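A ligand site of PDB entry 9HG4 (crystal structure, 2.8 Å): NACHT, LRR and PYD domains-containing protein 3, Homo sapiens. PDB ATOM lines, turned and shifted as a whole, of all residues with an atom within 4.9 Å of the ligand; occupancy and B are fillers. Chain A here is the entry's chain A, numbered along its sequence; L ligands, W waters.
Ala 98 touches the ligand. Pro 223 touches the ligand. Met 279 touches the ligand. CD1 of Ile 282 touches C10 of the ligand, 3.3 Å away. Val 285 touches the ligand. Thr 310 touches the ligand. OH of Tyr 314 touches C15 of the ligand (3.4 Å). CG2 of Thr 395 touches C14 of the ligand, 3.8 Å away. Ile 445 touches the ligand (CG2 to N2, 3.7 Å). CE2 of Phe 446 touches N2 of the ligand (3.2 Å). CE2 of Tyr 503 touches C8 of the ligand (3.5 Å). Met 532 touches the ligand (CE to C9, 3.5 Å). Hydrophobic or aromatic side chains that line the ligand: Ala 98, Ala 99, Pro 223, Met 279, Ile 282, Val 285, Tyr 314, Ile 445, Phe 446, Tyr 503 and Met 532. Of the 23 residues printed, 16 come within 4 Å of the ligand. Along chain A the residues within 4 Å of the ligand span positions 98 to 532.
The backbone carbonyl oxygen (O) of Ala 99 lies close to a nitrogen (N4) of the ligand. OE1 of Glu 500 lies within hydrogen-bond range of O1 of the ligand. The backbone NH (N) of Ala 99 lies within hydrogen-bond range of a nitrogen (N3) of the ligand (2.8 Å). An oxygen (O2) of the ligand lies within hydrogen-bond range of the guanidinium group (NE) of Arg 222 (2.8 Å). NH1 of Arg 449 lies within hydrogen-bond range of O3 of the ligand.
The guanidinium group of Arg 449 is in salt-bridge range of the side-chain carboxylate of Glu 500, 2.7 Å away. OH of Tyr 314 lies within hydrogen-bond range of OG1 of Thr 395 (2.6 Å). The side-chain hydroxyl (OG) of Ser 497 sits at hydrogen-bond distance from the backbone NH (N) of Glu 500.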
ATOM      1  N   GLY A  97     -33.924 -11.322   5.729  1.00  0.00           N
ATOM      2  CA  GLY A  97     -32.782 -11.523   4.847  1.00  0.00           C
ATOM      3  C   GLY A  97     -31.520 -10.940   5.419  1.00  0.00           C
ATOM      4  O   GLY A  97     -31.536  -9.850   6.000  1.00  0.00           O
ATOM      5  N   ALA A  98     -30.407 -11.632   5.227  1.00  0.00           N
ATOM      6  CA  ALA A  98     -29.112 -11.157   5.718  1.00  0.00           C
ATOM      7  C   ALA A  98     -28.742  -9.788   5.124  1.00  0.00           C
ATOM      8  O   ALA A  98     -29.277  -9.406   4.087  1.00  0.00           O
ATOM      9  CB  ALA A  98     -28.043 -12.184   5.377  1.00  0.00           C
ATOM     10  N   ALA A  99     -27.811  -9.042   5.758  1.00  0.00           N
ATOM     11  CA  ALA A  99     -27.387  -7.747   5.225  1.00  0.00           C
ATOM     12  C   ALA A  99     -26.758  -7.938   3.843  1.00  0.00           C
ATOM     13  O   ALA A  99     -26.019  -8.903   3.650  1.00  0.00           O
ATOM     14  CB  ALA A  99     -26.411  -7.069   6.170  1.00  0.00           C
ATOM     15  N   GLY A 100     -27.176  -7.132   2.890  1.00  0.00           N
ATOM     16  CA  GLY A 100     -26.706  -7.246   1.519  1.00  0.00           C
ATOM     17  C   GLY A 100     -27.381  -8.328   0.686  1.00  0.00           C
ATOM     18  O   GLY A 100     -27.019  -8.509  -0.472  1.00  0.00           O
ATOM     19  N   ARG A 222     -33.353  -7.624   8.638  1.00  0.00           N
ATOM     20  CA  ARG A 222     -32.216  -8.511   8.888  1.00  0.00           C
ATOM     21  C   ARG A 222     -32.675  -9.490   9.970  1.00  0.00           C
ATOM     22  O   ARG A 222     -33.426  -9.085  10.866  1.00  0.00           O
ATOM     23  CB  ARG A 222     -31.037  -7.712   9.424  1.00  0.00           C
ATOM     24  CG  ARG A 222     -30.218  -7.072   8.325  1.00  0.00           C
ATOM     25  CD  ARG A 222     -29.168  -6.119   8.871  1.00  0.00           C
ATOM     26  NE  ARG A 222     -28.262  -6.787   9.813  1.00  0.00           N
ATOM     27  CZ  ARG A 222     -27.370  -6.169  10.560  1.00  0.00           C
ATOM     28  NH1 ARG A 222     -26.604  -6.858  11.385  1.00  0.00           N
ATOM     29  NH2 ARG A 222     -27.262  -4.847  10.518  1.00  0.00           N
ATOM     30  N   PRO A 223     -32.240 -10.755   9.946  1.00  0.00           N
ATOM     31  CA  PRO A 223     -32.725 -11.716  10.947  1.00  0.00           C
ATOM     32  C   PRO A 223     -32.437 -11.333  12.397  1.00  0.00           C
ATOM     33  O   PRO A 223     -33.113 -11.815  13.312  1.00  0.00           O
ATOM     34  CB  PRO A 223     -32.033 -13.024  10.546  1.00  0.00           C
ATOM     35  CG  PRO A 223     -30.871 -12.597   9.712  1.00  0.00           C
ATOM     36  CD  PRO A 223     -31.338 -11.405   8.968  1.00  0.00           C
ATOM     37  N   VAL A 224     -31.463 -10.446  12.606  1.00  0.00           N
ATOM     38  CA  VAL A 224     -31.046  -9.961  13.915  1.00  0.00           C
ATOM     39  C   VAL A 224     -32.196  -9.175  14.608  1.00  0.00           C
ATOM     40  O   VAL A 224     -32.422  -9.327  15.818  1.00  0.00           O
ATOM     41  CB  VAL A 224     -29.706  -9.204  13.774  1.00  0.00           C
ATOM     42  CG1 VAL A 224     -29.852  -7.830  13.144  1.00  0.00           C
ATOM     43  CG2 VAL A 224     -28.951  -9.142  15.085  1.00  0.00           C
ATOM     44  N   MET A 279     -19.521 -17.213  -0.416  1.00  0.00           N
ATOM     45  CA  MET A 279     -20.016 -15.887  -0.048  1.00  0.00           C
ATOM     46  C   MET A 279     -20.841 -15.217  -1.122  1.00  0.00           C
ATOM     47  O   MET A 279     -21.580 -14.279  -0.815  1.00  0.00           O
ATOM     48  CB  MET A 279     -18.868 -14.945   0.245  1.00  0.00           C
ATOM     49  CG  MET A 279     -18.179 -15.218   1.519  1.00  0.00           C
ATOM     50  SD  MET A 279     -17.057 -13.861   1.903  1.00  0.00           S
ATOM     51  CE  MET A 279     -18.174 -12.571   2.081  1.00  0.00           C
ATOM     52  N   PHE A 281     -23.411 -16.033  -2.568  1.00  0.00           N
ATOM     53  CA  PHE A 281     -24.858 -16.180  -2.470  1.00  0.00           C
ATOM     54  C   PHE A 281     -25.451 -14.772  -2.075  1.00  0.00           C
ATOM     55  O   PHE A 281     -26.616 -14.498  -2.349  1.00  0.00           O
ATOM     56  CB  PHE A 281     -25.250 -17.262  -1.463  1.00  0.00           C
ATOM     57  CG  PHE A 281     -25.262 -16.851  -0.004  1.00  0.00           C
ATOM     58  CD1 PHE A 281     -24.098 -16.836   0.737  1.00  0.00           C
ATOM     59  CD2 PHE A 281     -26.445 -16.529   0.621  1.00  0.00           C
ATOM     60  CE1 PHE A 281     -24.110 -16.496   2.081  1.00  0.00           C
ATOM     61  CE2 PHE A 281     -26.455 -16.178   1.958  1.00  0.00           C
ATOM     62  CZ  PHE A 281     -25.284 -16.160   2.676  1.00  0.00           C
ATOM     63  N   ILE A 282     -24.649 -13.878  -1.451  1.00  0.00           N
ATOM     64  CA  ILE A 282     -25.054 -12.538  -1.087  1.00  0.00           C
ATOM     65  C   ILE A 282     -24.807 -11.621  -2.295  1.00  0.00           C
ATOM     66  O   ILE A 282     -23.660 -11.424  -2.703  1.00  0.00           O
ATOM     67  CB  ILE A 282     -24.226 -12.077   0.125  1.00  0.00           C
ATOM     68  CG1 ILE A 282     -24.480 -12.953   1.331  1.00  0.00           C
ATOM     69  CG2 ILE A 282     -24.471 -10.622   0.458  1.00  0.00           C
ATOM     70  CD1 ILE A 282     -23.349 -13.032   2.217  1.00  0.00           C
ATOM     71  N   LEU A 284     -24.691  -8.444  -2.605  1.00  0.00           N
ATOM     72  CA  LEU A 284     -23.766  -7.345  -2.310  1.00  0.00           C
ATOM     73  C   LEU A 284     -22.330  -7.858  -2.483  1.00  0.00           C
ATOM     74  O   LEU A 284     -21.520  -7.158  -3.074  1.00  0.00           O
ATOM     75  CB  LEU A 284     -23.984  -6.789  -0.897  1.00  0.00           C
ATOM     76  CG  LEU A 284     -22.980  -5.743  -0.435  1.00  0.00           C
ATOM     77  CD1 LEU A 284     -23.020  -4.516  -1.281  1.00  0.00           C
ATOM     78  CD2 LEU A 284     -23.189  -5.393   1.009  1.00  0.00           C
ATOM     79  N   VAL A 285     -22.045  -9.102  -2.045  1.00  0.00           N
ATOM     80  CA  VAL A 285     -20.736  -9.716  -2.222  1.00  0.00           C
ATOM     81  C   VAL A 285     -20.438  -9.876  -3.705  1.00  0.00           C
ATOM     82  O   VAL A 285     -19.355  -9.468  -4.139  1.00  0.00           O
ATOM     83  CB  VAL A 285     -20.591 -11.041  -1.428  1.00  0.00           C
ATOM     84  CG1 VAL A 285     -19.272 -11.733  -1.772  1.00  0.00           C
ATOM     85  CG2 VAL A 285     -20.712 -10.780   0.063  1.00  0.00           C
ATOM     86  N   THR A 310     -14.605 -12.081   5.079  1.00  0.00           N
ATOM     87  CA  THR A 310     -15.340 -10.925   4.563  1.00  0.00           C
ATOM     88  C   THR A 310     -14.465  -9.641   4.790  1.00  0.00           C
ATOM     89  O   THR A 310     -14.473  -8.789   3.927  1.00  0.00           O
ATOM     90  CB  THR A 310     -16.841 -10.824   4.991  1.00  0.00           C
ATOM     91  OG1 THR A 310     -17.140  -9.570   5.623  1.00  0.00           O
ATOM     92  CG2 THR A 310     -17.343 -11.992   5.833  1.00  0.00           C
ATOM     93  N   TYR A 314     -13.568  -6.977   1.850  1.00  0.00           N
ATOM     94  CA  TYR A 314     -13.799  -5.540   2.004  1.00  0.00           C
ATOM     95  C   TYR A 314     -12.522  -4.740   1.830  1.00  0.00           C
ATOM     96  O   TYR A 314     -12.546  -3.689   1.205  1.00  0.00           O
ATOM     97  CB  TYR A 314     -14.477  -5.212   3.336  1.00  0.00           C
ATOM     98  CG  TYR A 314     -15.988  -5.298   3.242  1.00  0.00           C
ATOM     99  CD1 TYR A 314     -16.616  -6.483   2.877  1.00  0.00           C
ATOM    100  CD2 TYR A 314     -16.778  -4.178   3.459  1.00  0.00           C
ATOM    101  CE1 TYR A 314     -17.993  -6.551   2.742  1.00  0.00           C
ATOM    102  CE2 TYR A 314     -18.163  -4.235   3.327  1.00  0.00           C
ATOM    103  CZ  TYR A 314     -18.756  -5.432   2.968  1.00  0.00           C
ATOM    104  OH  TYR A 314     -20.120  -5.521   2.815  1.00  0.00           O
ATOM    105  N   THR A 395     -22.941  -2.060   5.688  1.00  0.00           N
ATOM    106  CA  THR A 395     -21.771  -2.873   6.025  1.00  0.00           C
ATOM    107  C   THR A 395     -20.478  -2.057   5.871  1.00  0.00           C
ATOM    108  O   THR A 395     -19.542  -2.269   6.641  1.00  0.00           O
ATOM    109  CB  THR A 395     -21.741  -4.157   5.215  1.00  0.00           C
ATOM    110  OG1 THR A 395     -21.848  -3.836   3.843  1.00  0.00           O
ATOM    111  CG2 THR A 395     -22.843  -5.125   5.621  1.00  0.00           C
ATOM    112  N   ILE A 445     -23.075  -5.820  14.547  1.00  0.00           N
ATOM    113  CA  ILE A 445     -22.641  -7.134  14.091  1.00  0.00           C
ATOM    114  C   ILE A 445     -21.392  -7.040  13.233  1.00  0.00           C
ATOM    115  O   ILE A 445     -20.419  -7.745  13.490  1.00  0.00           O
ATOM    116  CB  ILE A 445     -23.773  -7.885  13.347  1.00  0.00           C
ATOM    117  CG1 ILE A 445     -25.046  -7.984  14.188  1.00  0.00           C
ATOM    118  CG2 ILE A 445     -23.303  -9.266  12.871  1.00  0.00           C
ATOM    119  CD1 ILE A 445     -24.962  -8.768  15.410  1.00  0.00           C
ATOM    120  N   PHE A 446     -21.408  -6.153  12.237  1.00  0.00           N
ATOM    121  CA  PHE A 446     -20.276  -5.995  11.350  1.00  0.00           C
ATOM    122  C   PHE A 446     -19.173  -5.198  11.960  1.00  0.00           C
ATOM    123  O   PHE A 446     -18.031  -5.473  11.644  1.00  0.00           O
ATOM    124  CB  PHE A 446     -20.687  -5.425   9.984  1.00  0.00           C
ATOM    125  CG  PHE A 446     -21.564  -6.379   9.227  1.00  0.00           C
ATOM    126  CD1 PHE A 446     -21.020  -7.449   8.536  1.00  0.00           C
ATOM    127  CD2 PHE A 446     -22.943  -6.246   9.262  1.00  0.00           C
ATOM    128  CE1 PHE A 446     -21.838  -8.360   7.893  1.00  0.00           C
ATOM    129  CE2 PHE A 446     -23.750  -7.156   8.609  1.00  0.00           C
ATOM    130  CZ  PHE A 446     -23.193  -8.205   7.947  1.00  0.00           C
ATOM    131  N   ARG A 449     -17.453  -7.955  13.903  1.00  0.00           N
ATOM    132  CA  ARG A 449     -16.844  -8.911  12.969  1.00  0.00           C
ATOM    133  C   ARG A 449     -15.611  -8.316  12.286  1.00  0.00           C
ATOM    134  O   ARG A 449     -14.609  -8.999  12.162  1.00  0.00           O
ATOM    135  CB  ARG A 449     -17.839  -9.327  11.883  1.00  0.00           C
ATOM    136  CG  ARG A 449     -18.789 -10.433  12.252  1.00  0.00           C
ATOM    137  CD  ARG A 449     -19.569 -10.780  11.011  1.00  0.00           C
ATOM    138  NE  ARG A 449     -20.750 -11.579  11.324  1.00  0.00           N
ATOM    139  CZ  ARG A 449     -21.668 -11.942  10.437  1.00  0.00           C
ATOM    140  NH1 ARG A 449     -21.535 -11.600   9.154  1.00  0.00           N
ATOM    141  NH2 ARG A 449     -22.714 -12.656  10.816  1.00  0.00           N
ATOM    142  N   SER A 497     -25.071 -15.355  19.175  1.00  0.00           N
ATOM    143  CA  SER A 497     -25.241 -16.802  19.177  1.00  0.00           C
ATOM    144  C   SER A 497     -23.868 -17.472  19.055  1.00  0.00           C
ATOM    145  O   SER A 497     -22.874 -16.807  18.762  1.00  0.00           O
ATOM    146  CB  SER A 497     -26.151 -17.242  18.035  1.00  0.00           C
ATOM    147  OG  SER A 497     -25.565 -16.957  16.774  1.00  0.00           O
ATOM    148  N   LEU A 499     -22.951 -19.544  16.715  1.00  0.00           N
ATOM    149  CA  LEU A 499     -22.629 -19.408  15.302  1.00  0.00           C
ATOM    150  C   LEU A 499     -22.118 -18.002  14.985  1.00  0.00           C
ATOM    151  O   LEU A 499     -21.187 -17.862  14.191  1.00  0.00           O
ATOM    152  CB  LEU A 499     -23.842 -19.732  14.429  1.00  0.00           C
ATOM    153  CG  LEU A 499     -23.612 -19.706  12.933  1.00  0.00           C
ATOM    154  CD1 LEU A 499     -22.552 -20.734  12.528  1.00  0.00           C
ATOM    155  CD2 LEU A 499     -24.888 -19.973  12.187  1.00  0.00           C
ATOM    156  N   GLU A 500     -22.656 -16.962  15.636  1.00  0.00           N
ATOM    157  CA  GLU A 500     -22.174 -15.596  15.431  1.00  0.00           C
ATOM    158  C   GLU A 500     -20.760 -15.469  15.954  1.00  0.00           C
ATOM    159  O   GLU A 500     -19.914 -14.883  15.273  1.00  0.00           O
ATOM    160  CB  GLU A 500     -23.112 -14.560  16.028  1.00  0.00           C
ATOM    161  CG  GLU A 500     -22.670 -13.136  15.763  1.00  0.00           C
ATOM    162  CD  GLU A 500     -22.449 -12.795  14.302  1.00  0.00           C
ATOM    163  OE1 GLU A 500     -23.275 -13.206  13.449  1.00  0.00           O
ATOM    164  OE2 GLU A 500     -21.439 -12.118  14.007  1.00  0.00           O
ATOM    165  N   TYR A 503     -18.555 -16.773  13.340  1.00  0.00           N
ATOM    166  CA  TYR A 503     -18.323 -15.815  12.247  1.00  0.00           C
ATOM    167  C   TYR A 503     -17.217 -14.818  12.626  1.00  0.00           C
ATOM    168  O   TYR A 503     -16.416 -14.438  11.778  1.00  0.00           O
ATOM    169  CB  TYR A 503     -19.617 -15.064  11.859  1.00  0.00           C
ATOM    170  CG  TYR A 503     -20.432 -15.776  10.804  1.00  0.00           C
ATOM    171  CD1 TYR A 503     -21.344 -16.752  11.155  1.00  0.00           C
ATOM    172  CD2 TYR A 503     -20.281 -15.470   9.464  1.00  0.00           C
ATOM    173  CE1 TYR A 503     -22.092 -17.418  10.192  1.00  0.00           C
ATOM    174  CE2 TYR A 503     -21.026 -16.124   8.493  1.00  0.00           C
ATOM    175  CZ  TYR A 503     -21.928 -17.095   8.857  1.00  0.00           C
ATOM    176  OH  TYR A 503     -22.675 -17.757   7.915  1.00  0.00           O
ATOM    177  N   MET A 532     -22.422 -21.203   3.976  1.00  0.00           N
ATOM    178  CA  MET A 532     -21.533 -20.248   4.651  1.00  0.00           C
ATOM    179  C   MET A 532     -21.419 -20.625   6.133  1.00  0.00           C
ATOM    180  O   MET A 532     -20.320 -20.560   6.689  1.00  0.00           O
ATOM    181  CB  MET A 532     -22.083 -18.824   4.553  1.00  0.00           C
ATOM    182  CG  MET A 532     -21.323 -17.927   3.619  1.00  0.00           C
ATOM    183  SD  MET A 532     -19.544 -17.781   3.871  1.00  0.00           S
ATOM    184  CE  MET A 532     -19.489 -17.188   5.446  1.00  0.00           C
HETATM  185  C1  LIG L   1     -25.072 -15.550  11.689  1.00  0.00           C
HETATM  186  C2  LIG L   1     -26.367 -14.833  12.074  1.00  0.00           C
HETATM  187  C3  LIG L   1     -27.526 -15.815  12.179  1.00  0.00           C
HETATM  188  C4  LIG L   1     -24.955 -10.885   7.436  1.00  0.00           C
HETATM  189  C5  LIG L   1     -23.366 -11.121   5.527  1.00  0.00           C
HETATM  190  C6  LIG L   1     -22.903 -12.447   5.623  1.00  0.00           C
HETATM  191  C7  LIG L   1     -23.612 -13.647   6.188  1.00  0.00           C
HETATM  192  C8  LIG L   1     -22.763 -14.824   5.721  1.00  0.00           C
HETATM  193  C9  LIG L   1     -21.394 -14.253   5.327  1.00  0.00           C
HETATM  194  C10 LIG L   1     -21.661 -12.794   5.092  1.00  0.00           C
HETATM  195  C11 LIG L   1     -20.873 -11.842   4.461  1.00  0.00           C
HETATM  196  C12 LIG L   1     -21.325 -10.531   4.354  1.00  0.00           C
HETATM  197  C13 LIG L   1     -22.567 -10.172   4.865  1.00  0.00           C
HETATM  198  C14 LIG L   1     -22.921  -8.752   4.529  1.00  0.00           C
HETATM  199  C15 LIG L   1     -21.801  -8.327   3.573  1.00  0.00           C
HETATM  200  C16 LIG L   1     -20.654  -9.344   3.724  1.00  0.00           C
HETATM  201  O1  LIG L   1     -26.170 -14.199  13.355  1.00  0.00           O
HETATM  202  C17 LIG L   1     -26.686 -13.774  11.034  1.00  0.00           C
HETATM  203  N1  LIG L   1     -27.251 -14.003   9.887  1.00  0.00           N
HETATM  204  C18 LIG L   1     -27.335 -12.844   9.153  1.00  0.00           C
HETATM  205  C19 LIG L   1     -26.832 -11.746   9.762  1.00  0.00           C
HETATM  206  S1  LIG L   1     -26.223 -12.078  11.303  1.00  0.00           S
HETATM  207  S2  LIG L   1     -26.714 -10.126   9.104  1.00  0.00           S
HETATM  208  N2  LIG L   1     -25.682  -9.302   9.977  1.00  0.00           N
HETATM  209  O2  LIG L   1     -28.009  -9.547   9.282  1.00  0.00           O
HETATM  210  N3  LIG L   1     -26.222 -10.328   7.685  1.00  0.00           N
HETATM  211  O3  LIG L   1     -24.266 -11.451   8.294  1.00  0.00           O
HETATM  212  N4  LIG L   1     -24.578 -10.730   6.150  1.00  0.00           N
HETATM  213  O   HOH W   1     -26.587 -16.486   8.676  1.00  0.00           O
